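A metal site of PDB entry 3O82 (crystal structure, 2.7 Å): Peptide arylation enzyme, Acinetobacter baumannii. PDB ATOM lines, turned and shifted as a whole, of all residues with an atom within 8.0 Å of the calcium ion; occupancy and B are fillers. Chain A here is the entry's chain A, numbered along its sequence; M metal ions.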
ATOM      1  N   VAL A 282       8.945   3.515  26.249  1.00  0.00           N
ATOM      2  CA  VAL A 282       8.918   3.976  27.634  1.00  0.00           C
ATOM      3  C   VAL A 282       7.476   4.000  28.155  1.00  0.00           C
ATOM      4  O   VAL A 282       6.588   4.560  27.504  1.00  0.00           O
ATOM      5  CB  VAL A 282       9.483   5.420  27.696  1.00  0.00           C
ATOM      6  CG1 VAL A 282       9.063   6.170  28.947  1.00  0.00           C
ATOM      7  CG2 VAL A 282      10.971   5.384  27.551  1.00  0.00           C
ATOM      8  N   ASN A 283       7.258   3.367  29.307  1.00  0.00           N
ATOM      9  CA  ASN A 283       5.914   3.332  29.883  1.00  0.00           C
ATOM     10  C   ASN A 283       5.770   4.145  31.182  1.00  0.00           C
ATOM     11  O   ASN A 283       4.673   4.244  31.735  1.00  0.00           O
ATOM     12  CB  ASN A 283       5.487   1.886  30.098  1.00  0.00           C
ATOM     13  CG  ASN A 283       6.536   1.049  30.836  1.00  0.00           C
ATOM     14  OD1 ASN A 283       7.335   1.538  31.641  1.00  0.00           O
ATOM     15  ND2 ASN A 283       6.502  -0.246  30.582  1.00  0.00           N
ATOM     16  N   LYS A 303       0.411  12.774  19.951  1.00  0.00           N
ATOM     17  CA  LYS A 303      -0.350  11.672  20.563  1.00  0.00           C
ATOM     18  C   LYS A 303       0.313  10.333  20.199  1.00  0.00           C
ATOM     19  O   LYS A 303       0.592   9.548  21.093  1.00  0.00           O
ATOM     20  CB  LYS A 303      -1.858  11.691  20.207  1.00  0.00           C
ATOM     21  N   ILE A 306       3.783   9.196  21.946  1.00  0.00           N
ATOM     22  CA  ILE A 306       3.814   8.968  23.429  1.00  0.00           C
ATOM     23  C   ILE A 306       2.747   8.034  24.029  1.00  0.00           C
ATOM     24  O   ILE A 306       2.601   7.977  25.232  1.00  0.00           O
ATOM     25  CB  ILE A 306       3.824  10.281  24.251  1.00  0.00           C
ATOM     26  CG1 ILE A 306       2.526  11.061  24.083  1.00  0.00           C
ATOM     27  CG2 ILE A 306       4.996  11.137  23.874  1.00  0.00           C
ATOM     28  CD1 ILE A 306       2.297  11.971  25.242  1.00  0.00           C
ATOM     29  N   GLN A 307       2.008   7.311  23.195  1.00  0.00           N
ATOM     30  CA  GLN A 307       0.981   6.395  23.658  1.00  0.00           C
ATOM     31  C   GLN A 307       1.503   5.380  24.683  1.00  0.00           C
ATOM     32  O   GLN A 307       0.842   5.114  25.661  1.00  0.00           O
ATOM     33  CB  GLN A 307       0.297   5.686  22.490  1.00  0.00           C
ATOM     34  CG  GLN A 307       1.238   4.812  21.654  1.00  0.00           C
ATOM     35  CD  GLN A 307       0.561   4.120  20.462  1.00  0.00           C
ATOM     36  OE1 GLN A 307      -0.296   3.249  20.637  1.00  0.00           O
ATOM     37  NE2 GLN A 307       0.980   4.490  19.237  1.00  0.00           N
ATOM     38  N   SER A 308       2.699   4.831  24.459  1.00  0.00           N
ATOM     39  CA  SER A 308       3.213   3.725  25.267  1.00  0.00           C
ATOM     40  C   SER A 308       3.282   4.040  26.750  1.00  0.00           C
ATOM     41  O   SER A 308       3.332   3.144  27.602  1.00  0.00           O
ATOM     42  CB  SER A 308       4.591   3.331  24.774  1.00  0.00           C
ATOM     43  OG  SER A 308       5.465   4.402  25.019  1.00  0.00           O
ATOM     44  N   LEU A 309       3.251   5.320  27.049  1.00  0.00           N
ATOM     45  CA  LEU A 309       3.371   5.851  28.382  1.00  0.00           C
ATOM     46  C   LEU A 309       2.176   5.455  29.202  1.00  0.00           C
ATOM     47  O   LEU A 309       1.040   5.685  28.803  1.00  0.00           O
ATOM     48  CB  LEU A 309       3.430   7.361  28.272  1.00  0.00           C
ATOM     49  CG  LEU A 309       4.018   8.260  29.345  1.00  0.00           C
ATOM     50  CD1 LEU A 309       5.545   7.965  29.556  1.00  0.00           C
ATOM     51  CD2 LEU A 309       3.780   9.704  28.928  1.00  0.00           C
ATOM     52  N   LYS A 310       2.429   4.872  30.364  1.00  0.00           N
ATOM     53  CA  LYS A 310       1.355   4.367  31.169  1.00  0.00           C
ATOM     54  C   LYS A 310       1.221   5.118  32.489  1.00  0.00           C
ATOM     55  O   LYS A 310       0.146   5.096  33.071  1.00  0.00           O
ATOM     56  CB  LYS A 310       1.590   2.911  31.513  1.00  0.00           C
ATOM     57  CG  LYS A 310       1.579   1.931  30.380  1.00  0.00           C
ATOM     58  CD  LYS A 310       1.626   0.521  30.980  1.00  0.00           C
ATOM     59  CE  LYS A 310       1.972  -0.550  29.974  1.00  0.00           C
ATOM     60  NZ  LYS A 310       1.761  -1.879  30.589  1.00  0.00           N
ATOM     61  N   LEU A 311       2.306   5.707  32.985  1.00  0.00           N
ATOM     62  CA  LEU A 311       2.271   6.415  34.284  1.00  0.00           C
ATOM     63  C   LEU A 311       3.224   7.588  34.313  1.00  0.00           C
ATOM     64  O   LEU A 311       4.374   7.488  33.882  1.00  0.00           O
ATOM     65  CB  LEU A 311       2.581   5.464  35.434  1.00  0.00           C
ATOM     66  CG  LEU A 311       2.730   5.980  36.875  1.00  0.00           C
ATOM     67  CD1 LEU A 311       1.408   6.440  37.463  1.00  0.00           C
ATOM     68  CD2 LEU A 311       3.341   4.891  37.768  1.00  0.00           C
ATOM     69  N   PRO A 328      -4.189  13.022  32.526  1.00  0.00           N
ATOM     70  CA  PRO A 328      -4.815  11.898  31.835  1.00  0.00           C
ATOM     71  C   PRO A 328      -5.436  12.233  30.482  1.00  0.00           C
ATOM     72  O   PRO A 328      -5.270  11.451  29.546  1.00  0.00           O
ATOM     73  CB  PRO A 328      -5.887  11.433  32.815  1.00  0.00           C
ATOM     74  CG  PRO A 328      -6.070  12.578  33.755  1.00  0.00           C
ATOM     75  CD  PRO A 328      -4.720  13.134  33.897  1.00  0.00           C
ATOM     76  N   LEU A 331      -2.089  13.651  28.226  1.00  0.00           N
ATOM     77  CA  LEU A 331      -0.890  12.804  28.121  1.00  0.00           C
ATOM     78  C   LEU A 331      -1.234  11.331  27.933  1.00  0.00           C
ATOM     79  O   LEU A 331      -0.397  10.512  27.518  1.00  0.00           O
ATOM     80  CB  LEU A 331       0.091  13.055  29.288  1.00  0.00           C
ATOM     81  CG  LEU A 331       0.705  14.464  29.390  1.00  0.00           C
ATOM     82  CD1 LEU A 331       1.730  14.599  30.490  1.00  0.00           C
ATOM     83  CD2 LEU A 331       1.322  14.797  28.073  1.00  0.00           C
ATOM     84  N   ASN A 332      -2.481  11.003  28.224  1.00  0.00           N
ATOM     85  CA  ASN A 332      -2.991   9.651  28.056  1.00  0.00           C
ATOM     86  C   ASN A 332      -2.244   8.644  28.923  1.00  0.00           C
ATOM     87  O   ASN A 332      -1.704   7.680  28.428  1.00  0.00           O
ATOM     88  CB  ASN A 332      -2.974   9.221  26.583  1.00  0.00           C
ATOM     89  CG  ASN A 332      -3.797  10.129  25.675  1.00  0.00           C
ATOM     90  OD1 ASN A 332      -4.756  10.790  26.094  1.00  0.00           O
ATOM     91  ND2 ASN A 332      -3.435  10.147  24.418  1.00  0.00           N
ATOM     92  N   CYS A 333      -2.219   8.906  30.217  1.00  0.00           N
ATOM     93  CA  CYS A 333      -1.615   8.009  31.184  1.00  0.00           C
ATOM     94  C   CYS A 333      -2.083   8.312  32.578  1.00  0.00           C
ATOM     95  O   CYS A 333      -2.642   9.344  32.849  1.00  0.00           O
ATOM     96  CB  CYS A 333      -0.104   8.120  31.120  1.00  0.00           C
ATOM     97  SG  CYS A 333       0.543   9.712  31.644  1.00  0.00           S
ATOM     98  N   LYS A 334      -1.846   7.412  33.496  1.00  0.00           N
ATOM     99  CA  LYS A 334      -2.326   7.572  34.841  1.00  0.00           C
ATOM    100  C   LYS A 334      -1.511   8.676  35.492  1.00  0.00           C
ATOM    101  O   LYS A 334      -0.363   8.857  35.156  1.00  0.00           O
ATOM    102  CB  LYS A 334      -2.158   6.235  35.579  1.00  0.00           C
ATOM    103  CG  LYS A 334      -2.356   6.250  37.074  1.00  0.00           C
ATOM    104  CD  LYS A 334      -3.828   6.229  37.462  1.00  0.00           C
ATOM    105  CE  LYS A 334      -4.015   5.397  38.705  1.00  0.00           C
ATOM    106  NZ  LYS A 334      -5.443   5.413  39.041  1.00  0.00           N
HETATM  107 CA    CA M   1      -0.723   5.718  27.193  1.00  0.00          CA
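The backbone NH of Leu 309 lies within hydrogen-bond range of the backbone carbonyl oxygen of Val 282 (3.5 Å).
Of the 14 residues printed, 3 come within 4 Å of the calcium ion. Along chain A the residues within 4 Å of the calcium ion span positions 307 to 332. The nearest printed residue that does not touch the calcium ion is Ser 308 (4.4 Å).
The calcium ion is bound by O of Gln 307 (2.3 Å), O of Leu 309 (2.4 Å) and O of Asn 332 (2.5 Å).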
